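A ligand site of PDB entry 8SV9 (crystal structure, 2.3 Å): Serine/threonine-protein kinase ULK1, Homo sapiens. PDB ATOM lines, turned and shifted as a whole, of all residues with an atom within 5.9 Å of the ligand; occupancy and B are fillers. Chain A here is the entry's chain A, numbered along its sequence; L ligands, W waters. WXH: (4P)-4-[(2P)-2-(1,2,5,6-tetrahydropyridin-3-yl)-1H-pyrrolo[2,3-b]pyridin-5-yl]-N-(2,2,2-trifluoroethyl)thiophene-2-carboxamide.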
ATOM      1  N   ILE A  22      14.824  -2.675 -23.934  1.00  0.00           N
ATOM      2  CA  ILE A  22      14.112  -3.610 -24.796  1.00  0.00           C
ATOM      3  C   ILE A  22      12.608  -3.360 -24.800  1.00  0.00           C
ATOM      4  O   ILE A  22      11.872  -4.086 -25.460  1.00  0.00           O
ATOM      5  CB  ILE A  22      14.400  -5.078 -24.414  1.00  0.00           C
ATOM      6  CG1 ILE A  22      13.816  -5.387 -23.036  1.00  0.00           C
ATOM      7  CG2 ILE A  22      15.904  -5.343 -24.437  1.00  0.00           C
ATOM      8  CD1 ILE A  22      14.202  -6.742 -22.507  1.00  0.00           C
ATOM      9  N   GLY A  23      12.139  -2.340 -24.081  1.00  0.00           N
ATOM     10  CA  GLY A  23      10.725  -2.035 -24.025  1.00  0.00           C
ATOM     11  C   GLY A  23      10.433  -0.887 -23.081  1.00  0.00           C
ATOM     12  O   GLY A  23      11.135  -0.708 -22.084  1.00  0.00           O
ATOM     13  N   HIS A  24       9.414  -0.097 -23.390  1.00  0.00           N
ATOM     14  CA  HIS A  24       9.093   1.049 -22.553  1.00  0.00           C
ATOM     15  C   HIS A  24       7.638   1.438 -22.752  1.00  0.00           C
ATOM     16  O   HIS A  24       7.048   1.184 -23.814  1.00  0.00           O
ATOM     17  CB  HIS A  24       9.998   2.243 -22.846  1.00  0.00           C
ATOM     18  CG  HIS A  24       9.737   2.871 -24.186  1.00  0.00           C
ATOM     19  ND1 HIS A  24       9.042   4.055 -24.334  1.00  0.00           N
ATOM     20  CD2 HIS A  24      10.090   2.484 -25.442  1.00  0.00           C
ATOM     21  CE1 HIS A  24       8.975   4.371 -25.611  1.00  0.00           C
ATOM     22  NE2 HIS A  24       9.602   3.434 -26.300  1.00  0.00           N
ATOM     23  N   GLY A  25       7.063   2.065 -21.724  1.00  0.00           N
ATOM     24  CA  GLY A  25       5.726   2.595 -21.793  1.00  0.00           C
ATOM     25  C   GLY A  25       5.653   3.907 -21.039  1.00  0.00           C
ATOM     26  O   GLY A  25       6.663   4.424 -20.543  1.00  0.00           O
ATOM     27  N   ALA A  26       4.435   4.444 -20.959  1.00  0.00           N
ATOM     28  CA  ALA A  26       4.214   5.688 -20.236  1.00  0.00           C
ATOM     29  C   ALA A  26       4.427   5.527 -18.737  1.00  0.00           C
ATOM     30  O   ALA A  26       4.689   6.525 -18.054  1.00  0.00           O
ATOM     31  CB  ALA A  26       2.798   6.206 -20.510  1.00  0.00           C
ATOM     32  N   ALA A  28       6.280   2.561 -17.351  1.00  0.00           N
ATOM     33  CA  ALA A  28       7.213   1.484 -17.061  1.00  0.00           C
ATOM     34  C   ALA A  28       8.349   1.512 -18.077  1.00  0.00           C
ATOM     35  O   ALA A  28       8.180   1.975 -19.203  1.00  0.00           O
ATOM     36  CB  ALA A  28       6.532   0.119 -17.070  1.00  0.00           C
ATOM     37  N   VAL A  29       9.494   0.996 -17.656  1.00  0.00           N
ATOM     38  CA  VAL A  29      10.681   0.876 -18.496  1.00  0.00           C
ATOM     39  C   VAL A  29      11.249  -0.527 -18.308  1.00  0.00           C
ATOM     40  O   VAL A  29      11.230  -1.071 -17.198  1.00  0.00           O
ATOM     41  CB  VAL A  29      11.704   1.982 -18.171  1.00  0.00           C
ATOM     42  CG1 VAL A  29      12.754   1.514 -17.172  1.00  0.00           C
ATOM     43  CG2 VAL A  29      12.354   2.508 -19.431  1.00  0.00           C
ATOM     44  N   VAL A  30      11.714  -1.131 -19.396  1.00  0.00           N
ATOM     45  CA  VAL A  30      12.164  -2.516 -19.389  1.00  0.00           C
ATOM     46  C   VAL A  30      13.559  -2.585 -20.005  1.00  0.00           C
ATOM     47  O   VAL A  30      13.779  -2.101 -21.116  1.00  0.00           O
ATOM     48  CB  VAL A  30      11.201  -3.439 -20.162  1.00  0.00           C
ATOM     49  CG1 VAL A  30      11.570  -4.901 -19.893  1.00  0.00           C
ATOM     50  CG2 VAL A  30       9.765  -3.177 -19.776  1.00  0.00           C
ATOM     51  N   ALA A  44      14.270  -9.901 -18.185  1.00  0.00           N
ATOM     52  CA  ALA A  44      13.832  -8.540 -18.475  1.00  0.00           C
ATOM     53  C   ALA A  44      13.505  -7.871 -17.150  1.00  0.00           C
ATOM     54  O   ALA A  44      12.647  -8.365 -16.397  1.00  0.00           O
ATOM     55  CB  ALA A  44      12.628  -8.536 -19.406  1.00  0.00           C
ATOM     56  N   LYS A  46      11.921  -4.833 -15.220  1.00  0.00           N
ATOM     57  CA  LYS A  46      10.937  -3.757 -15.354  1.00  0.00           C
ATOM     58  C   LYS A  46      11.096  -2.770 -14.209  1.00  0.00           C
ATOM     59  O   LYS A  46      11.085  -3.174 -13.032  1.00  0.00           O
ATOM     60  CB  LYS A  46       9.515  -4.325 -15.379  1.00  0.00           C
ATOM     61  CG  LYS A  46       8.443  -3.337 -15.783  1.00  0.00           C
ATOM     62  CD  LYS A  46       7.104  -4.045 -15.967  1.00  0.00           C
ATOM     63  CE  LYS A  46       6.261  -3.375 -17.045  1.00  0.00           C
ATOM     64  NZ  LYS A  46       4.814  -3.680 -16.902  1.00  0.00           N
ATOM     65  N   GLU A  63       0.913  -4.885 -10.596  1.00  0.00           N
ATOM     66  CA  GLU A  63       1.303  -5.969 -11.474  1.00  0.00           C
ATOM     67  C   GLU A  63       1.964  -7.116 -10.704  1.00  0.00           C
ATOM     68  O   GLU A  63       1.753  -8.288 -11.025  1.00  0.00           O
ATOM     69  CB  GLU A  63       2.252  -5.453 -12.561  1.00  0.00           C
ATOM     70  CG  GLU A  63       2.603  -6.496 -13.612  1.00  0.00           C
ATOM     71  CD  GLU A  63       3.342  -5.913 -14.799  1.00  0.00           C
ATOM     72  OE1 GLU A  63       3.876  -4.788 -14.678  1.00  0.00           O
ATOM     73  OE2 GLU A  63       3.368  -6.563 -15.858  1.00  0.00           O
ATOM     74  N   VAL A  76       3.682 -14.007 -19.233  1.00  0.00           N
ATOM     75  CA  VAL A  76       5.065 -13.643 -18.920  1.00  0.00           C
ATOM     76  C   VAL A  76       5.372 -14.027 -17.480  1.00  0.00           C
ATOM     77  O   VAL A  76       4.602 -13.732 -16.560  1.00  0.00           O
ATOM     78  CB  VAL A  76       5.296 -12.150 -19.180  1.00  0.00           C
ATOM     79  CG1 VAL A  76       4.309 -11.293 -18.373  1.00  0.00           C
ATOM     80  CG2 VAL A  76       6.739 -11.765 -18.890  1.00  0.00           C
ATOM     81  N   MET A  92      11.615 -10.331 -14.818  1.00  0.00           N
ATOM     82  CA  MET A  92      10.630 -11.056 -15.594  1.00  0.00           C
ATOM     83  C   MET A  92      11.288 -11.853 -16.714  1.00  0.00           C
ATOM     84  O   MET A  92      12.467 -11.693 -17.031  1.00  0.00           O
ATOM     85  CB  MET A  92       9.590 -10.098 -16.180  1.00  0.00           C
ATOM     86  CG  MET A  92       9.268  -8.926 -15.281  1.00  0.00           C
ATOM     87  SD  MET A  92       7.829  -8.046 -15.891  1.00  0.00           S
ATOM     88  CE  MET A  92       6.606  -9.330 -15.685  1.00  0.00           C
ATOM     89  N   GLU A  93      10.473 -12.717 -17.320  1.00  0.00           N
ATOM     90  CA  GLU A  93      10.912 -13.577 -18.401  1.00  0.00           C
ATOM     91  C   GLU A  93      11.347 -12.744 -19.611  1.00  0.00           C
ATOM     92  O   GLU A  93      10.716 -11.746 -19.956  1.00  0.00           O
ATOM     93  CB  GLU A  93       9.787 -14.540 -18.788  1.00  0.00           C
ATOM     94  CG  GLU A  93      10.016 -15.334 -20.061  1.00  0.00           C
ATOM     95  CD  GLU A  93       8.901 -16.316 -20.333  1.00  0.00           C
ATOM     96  OE1 GLU A  93       7.795 -16.135 -19.781  1.00  0.00           O
ATOM     97  OE2 GLU A  93       9.129 -17.273 -21.102  1.00  0.00           O
ATOM     98  N   TYR A  94      12.437 -13.166 -20.235  1.00  0.00           N
ATOM     99  CA  TYR A  94      12.906 -12.570 -21.474  1.00  0.00           C
ATOM    100  C   TYR A  94      12.425 -13.400 -22.656  1.00  0.00           C
ATOM    101  O   TYR A  94      12.432 -14.631 -22.608  1.00  0.00           O
ATOM    102  CB  TYR A  94      14.435 -12.473 -21.493  1.00  0.00           C
ATOM    103  CG  TYR A  94      14.985 -11.908 -22.786  1.00  0.00           C
ATOM    104  CD1 TYR A  94      14.938 -10.547 -23.051  1.00  0.00           C
ATOM    105  CD2 TYR A  94      15.553 -12.749 -23.746  1.00  0.00           C
ATOM    106  CE1 TYR A  94      15.448 -10.030 -24.227  1.00  0.00           C
ATOM    107  CE2 TYR A  94      16.063 -12.239 -24.929  1.00  0.00           C
ATOM    108  CZ  TYR A  94      16.005 -10.876 -25.165  1.00  0.00           C
ATOM    109  OH  TYR A  94      16.505 -10.373 -26.340  1.00  0.00           O
ATOM    110  N   CYS A  95      12.002 -12.723 -23.717  1.00  0.00           N
ATOM    111  CA  CYS A  95      11.478 -13.371 -24.915  1.00  0.00           C
ATOM    112  C   CYS A  95      12.329 -12.950 -26.109  1.00  0.00           C
ATOM    113  O   CYS A  95      12.345 -11.775 -26.478  1.00  0.00           O
ATOM    114  CB  CYS A  95      10.004 -13.004 -25.120  1.00  0.00           C
ATOM    115  SG  CYS A  95       8.943 -13.526 -23.749  1.00  0.00           S
ATOM    116  N   ASN A  96      13.037 -13.920 -26.695  1.00  0.00           N
ATOM    117  CA  ASN A  96      13.989 -13.608 -27.758  1.00  0.00           C
ATOM    118  C   ASN A  96      13.320 -13.130 -29.038  1.00  0.00           C
ATOM    119  O   ASN A  96      13.986 -12.517 -29.873  1.00  0.00           O
ATOM    120  CB  ASN A  96      14.858 -14.836 -28.066  1.00  0.00           C
ATOM    121  CG  ASN A  96      14.046 -16.101 -28.213  1.00  0.00           C
ATOM    122  OD1 ASN A  96      12.816 -16.082 -28.202  1.00  0.00           O
ATOM    123  ND2 ASN A  96      14.733 -17.233 -28.360  1.00  0.00           N
ATOM    124  N   GLY A  97      12.024 -13.389 -29.210  1.00  0.00           N
ATOM    125  CA  GLY A  97      11.336 -12.997 -30.419  1.00  0.00           C
ATOM    126  C   GLY A  97      10.796 -11.588 -30.458  1.00  0.00           C
ATOM    127  O   GLY A  97      10.327 -11.145 -31.521  1.00  0.00           O
ATOM    128  N   GLY A  98      10.840 -10.861 -29.348  1.00  0.00           N
ATOM    129  CA  GLY A  98      10.281  -9.524 -29.303  1.00  0.00           C
ATOM    130  C   GLY A  98       8.780  -9.542 -29.113  1.00  0.00           C
ATOM    131  O   GLY A  98       8.172 -10.580 -28.795  1.00  0.00           O
ATOM    132  N   ASP A  99       8.165  -8.389 -29.315  1.00  0.00           N
ATOM    133  CA  ASP A  99       6.723  -8.304 -29.170  1.00  0.00           C
ATOM    134  C   ASP A  99       6.033  -8.499 -30.521  1.00  0.00           C
ATOM    135  O   ASP A  99       6.660  -8.496 -31.581  1.00  0.00           O
ATOM    136  CB  ASP A  99       6.300  -6.965 -28.548  1.00  0.00           C
ATOM    137  CG  ASP A  99       6.768  -5.763 -29.343  1.00  0.00           C
ATOM    138  OD1 ASP A  99       6.373  -5.627 -30.521  1.00  0.00           O
ATOM    139  OD2 ASP A  99       7.513  -4.931 -28.776  1.00  0.00           O
ATOM    140  N   ASP A 102       6.371  -5.675 -33.334  1.00  0.00           N
ATOM    141  CA  ASP A 102       7.556  -5.696 -34.183  1.00  0.00           C
ATOM    142  C   ASP A 102       7.478  -6.814 -35.217  1.00  0.00           C
ATOM    143  O   ASP A 102       7.913  -6.642 -36.356  1.00  0.00           O
ATOM    144  CB  ASP A 102       8.814  -5.861 -33.322  1.00  0.00           C
ATOM    145  CG  ASP A 102       9.132  -4.630 -32.495  1.00  0.00           C
ATOM    146  OD1 ASP A 102       8.608  -3.536 -32.826  1.00  0.00           O
ATOM    147  OD2 ASP A 102       9.897  -4.742 -31.522  1.00  0.00           O
ATOM    148  N   GLN A 142       1.862  -4.847 -28.817  1.00  0.00           N
ATOM    149  CA  GLN A 142       3.042  -4.496 -28.044  1.00  0.00           C
ATOM    150  C   GLN A 142       3.125  -5.278 -26.742  1.00  0.00           C
ATOM    151  O   GLN A 142       4.215  -5.495 -26.212  1.00  0.00           O
ATOM    152  CB  GLN A 142       3.039  -2.981 -27.761  1.00  0.00           C
ATOM    153  CG  GLN A 142       4.298  -2.459 -27.079  1.00  0.00           C
ATOM    154  CD  GLN A 142       4.007  -1.344 -26.098  1.00  0.00           C
ATOM    155  OE1 GLN A 142       3.574  -0.253 -26.470  1.00  0.00           O
ATOM    156  NE2 GLN A 142       4.253  -1.600 -24.811  1.00  0.00           N
ATOM    157  N   ASN A 143       1.978  -5.724 -26.208  1.00  0.00           N
ATOM    158  CA  ASN A 143       1.941  -6.477 -24.959  1.00  0.00           C
ATOM    159  C   ASN A 143       1.834  -7.981 -25.194  1.00  0.00           C
ATOM    160  O   ASN A 143       1.588  -8.734 -24.245  1.00  0.00           O
ATOM    161  CB  ASN A 143       0.769  -6.000 -24.093  1.00  0.00           C
ATOM    162  CG  ASN A 143       1.017  -4.626 -23.498  1.00  0.00           C
ATOM    163  OD1 ASN A 143       2.160  -4.171 -23.422  1.00  0.00           O
ATOM    164  ND2 ASN A 143      -0.045  -3.958 -23.073  1.00  0.00           N
ATOM    165  N   LEU A 145       4.133 -11.056 -26.321  1.00  0.00           N
ATOM    166  CA  LEU A 145       5.539 -11.391 -26.481  1.00  0.00           C
ATOM    167  C   LEU A 145       5.692 -12.739 -27.161  1.00  0.00           C
ATOM    168  O   LEU A 145       4.874 -13.644 -26.990  1.00  0.00           O
ATOM    169  CB  LEU A 145       6.251 -11.394 -25.128  1.00  0.00           C
ATOM    170  CG  LEU A 145       6.398 -10.048 -24.425  1.00  0.00           C
ATOM    171  CD1 LEU A 145       7.143 -10.202 -23.108  1.00  0.00           C
ATOM    172  CD2 LEU A 145       7.100  -9.043 -25.321  1.00  0.00           C
ATOM    173  N   ARG A 152      15.793 -17.481 -32.696  1.00  0.00           N
ATOM    174  CA  ARG A 152      14.987 -16.291 -32.931  1.00  0.00           C
ATOM    175  C   ARG A 152      14.514 -16.180 -34.377  1.00  0.00           C
ATOM    176  O   ARG A 152      13.575 -15.420 -34.647  1.00  0.00           O
ATOM    177  CB  ARG A 152      15.778 -15.041 -32.534  1.00  0.00           C
ATOM    178  CG  ARG A 152      16.495 -14.356 -33.687  1.00  0.00           C
ATOM    179  CD  ARG A 152      16.953 -12.954 -33.307  1.00  0.00           C
ATOM    180  NE  ARG A 152      15.890 -11.964 -33.434  1.00  0.00           N
ATOM    181  CZ  ARG A 152      15.632 -11.019 -32.544  1.00  0.00           C
ATOM    182  NH1 ARG A 152      16.353 -10.895 -31.449  1.00  0.00           N
ATOM    183  NH2 ARG A 152      14.631 -10.171 -32.765  1.00  0.00           N
ATOM    184  N   ALA A 164       1.781 -10.061 -21.689  1.00  0.00           N
ATOM    185  CA  ALA A 164       2.565  -9.270 -20.765  1.00  0.00           C
ATOM    186  C   ALA A 164       1.785  -8.029 -20.329  1.00  0.00           C
ATOM    187  O   ALA A 164       0.654  -7.797 -20.754  1.00  0.00           O
ATOM    188  CB  ALA A 164       3.913  -8.878 -21.384  1.00  0.00           C
ATOM    189  N   ASP A 165       2.419  -7.237 -19.455  1.00  0.00           N
ATOM    190  CA  ASP A 165       1.908  -5.947 -18.979  1.00  0.00           C
ATOM    191  C   ASP A 165       0.575  -6.067 -18.262  1.00  0.00           C
ATOM    192  O   ASP A 165      -0.485  -5.789 -18.833  1.00  0.00           O
ATOM    193  CB  ASP A 165       1.791  -4.962 -20.150  1.00  0.00           C
ATOM    194  CG  ASP A 165       1.959  -3.524 -19.710  1.00  0.00           C
ATOM    195  OD1 ASP A 165       2.088  -3.298 -18.487  1.00  0.00           O
ATOM    196  OD2 ASP A 165       1.951  -2.633 -20.581  1.00  0.00           O
ATOM    197  N   PHE A 166       0.613  -6.448 -16.987  1.00  0.00           N
ATOM    198  CA  PHE A 166      -0.590  -6.643 -16.178  1.00  0.00           C
ATOM    199  C   PHE A 166      -0.831  -5.499 -15.198  1.00  0.00           C
ATOM    200  O   PHE A 166      -1.585  -5.661 -14.231  1.00  0.00           O
ATOM    201  CB  PHE A 166      -0.515  -7.985 -15.438  1.00  0.00           C
ATOM    202  CG  PHE A 166      -0.834  -9.162 -16.299  1.00  0.00           C
ATOM    203  CD1 PHE A 166       0.068  -9.627 -17.232  1.00  0.00           C
ATOM    204  CD2 PHE A 166      -2.056  -9.814 -16.174  1.00  0.00           C
ATOM    205  CE1 PHE A 166      -0.232 -10.715 -18.043  1.00  0.00           C
ATOM    206  CE2 PHE A 166      -2.366 -10.901 -16.971  1.00  0.00           C
ATOM    207  CZ  PHE A 166      -1.444 -11.359 -17.912  1.00  0.00           C
HETATM  208  C10 WXH L   1       8.124  -6.539 -21.751  1.00  0.00           C
HETATM  209  C13 WXH L   1      10.436  -7.268 -23.752  1.00  0.00           C
HETATM  210  C15 WXH L   1      11.826  -9.007 -24.638  1.00  0.00           C
HETATM  211  C17 WXH L   1      10.629  -9.428 -22.645  1.00  0.00           C
HETATM  212  C20 WXH L   1      13.531  -8.012 -27.733  1.00  0.00           C
HETATM  213  C21 WXH L   1      13.427  -6.694 -28.570  1.00  0.00           C
HETATM  214  C22 WXH L   1      14.114  -6.612 -29.800  1.00  0.00           C
HETATM  215  C26 WXH L   1      11.888  -7.189 -25.892  1.00  0.00           C
HETATM  216  C02 WXH L   1       6.268  -5.289 -20.359  1.00  0.00           C
HETATM  217  C04 WXH L   1       5.114  -3.171 -21.314  1.00  0.00           C
HETATM  218  C05 WXH L   1       5.875  -1.857 -21.165  1.00  0.00           C
HETATM  219  C09 WXH L   1       7.344  -6.354 -20.531  1.00  0.00           C
HETATM  220  C11 WXH L   1       9.088  -7.674 -21.563  1.00  0.00           C
HETATM  221  C12 WXH L   1      10.092  -8.155 -22.693  1.00  0.00           C
HETATM  222  C14 WXH L   1      11.329  -7.731 -24.750  1.00  0.00           C
HETATM  223  C19 WXH L   1      12.715  -8.163 -26.456  1.00  0.00           C
HETATM  224  C23 WXH L   1      15.251  -7.791 -29.989  1.00  0.00           C
HETATM  225  C25 WXH L   1      14.190  -9.171 -28.283  1.00  0.00           C
HETATM  226  C27 WXH L   1       8.958  -8.244 -20.224  1.00  0.00           C
HETATM  227  F06 WXH L   1       6.769  -1.724 -22.249  1.00  0.00           F
HETATM  228  F07 WXH L   1       4.959  -0.784 -21.171  1.00  0.00           F
HETATM  229  F08 WXH L   1       6.578  -1.877 -20.009  1.00  0.00           F
HETATM  230  N03 WXH L   1       6.129  -4.246 -21.428  1.00  0.00           N
HETATM  231  N16 WXH L   1      11.471  -9.832 -23.605  1.00  0.00           N
HETATM  232  N18 WXH L   1      12.655  -9.221 -25.699  1.00  0.00           N
HETATM  233  N24 WXH L   1      14.727  -8.981 -29.800  1.00  0.00           N
HETATM  234  O01 WXH L   1       5.551  -5.273 -19.387  1.00  0.00           O
HETATM  235  S28 WXH L   1       7.802  -7.431 -19.414  1.00  0.00           S
HETATM  236  O   HOH W   1      16.719  -7.343 -27.292  1.00  0.00           O
HETATM  237  O   HOH W   2       3.622  -0.876 -18.128  1.00  0.00           O
HETATM  238  O   HOH W   3       4.646  -7.712 -17.880  1.00  0.00           O
HETATM  239  O   HOH W   4       3.418   1.522 -19.689  1.00  0.00           O
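The backbone NH (N) of Cys 95 sits at hydrogen-bond distance from a nitrogen (N16) of the ligand (2.9 Å). O of Cys 95 sits at hydrogen-bond distance from N18 of the ligand (2.7 Å). A nitrogen (N24) of the ligand sits close to the guanidinium group of Arg 152, 3.0 Å away. The side-chain amino group (NZ) of Lys 46 lies within hydrogen-bond range of an oxygen (O01) of the ligand.
O of Asn 96 lies within hydrogen-bond range of NH1 of Arg 152, 3.3 Å away. NZ of Lys 46 lies within salt-bridge range of OD1 of Asp 165 (3.2 Å). The side-chain amino group (NZ) of Lys 46 lies within salt-bridge range of the side-chain carboxylate (OE1) of Glu 63 (2.7 Å). The backbone carbonyl oxygen of Val 30 lies within hydrogen-bond range of the backbone NH of Ile 22. The side-chain carboxylate of Asp 165 sits close to the side-chain amide oxygen of Asn 143, 3.2 Å away. N of Val 30 is in hydrogen-bond range of O of Gly 23, 2.8 Å away. The backbone NH (N) of Met 92 is in hydrogen-bond range of the backbone carbonyl oxygen (O) of Ala 44. The backbone NH of Ala 164 lies within hydrogen-bond range of the backbone carbonyl oxygen of Asn 143, 2.9 Å away.
Water W2 lies within hydrogen-bond range of OD1 of Asp 165 and NZ of Lys 46.
The backbone NH (N) of His 24 sits close to a fluorine (F06) of the ligand, 3.3 Å away. The side-chain sulfur of Met 92 lies close to a sulfur (S28) of the ligand. Residues that only touch the ligand: Ile 22 (3.1 Å), Gly 23 (3.8 Å), Gly 25 (3.5 Å), Ala 28 (3.6 Å), Val 30 (3.4 Å), Ala 44 (3.8 Å), Glu 93 (3.6 Å), Tyr 94 (3.3 Å), Asn 96 (3.6 Å), Gly 98 (3.9 Å), Gln 142 (3.6 Å), Asn 143 (3.8 Å), Leu 145 (3.5 Å) and Asp 165 (3.3 Å). Hydrophobic or aromatic side chains that line the ligand: Ile 22, Ala 28, Val 30, Ala 44, Met 92, Tyr 94 and Leu 145. Of the 28 residues printed, 19 come within 4 Å of the ligand. The nearest printed residue that does not touch the ligand is Ala 164 (4.3 Å).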
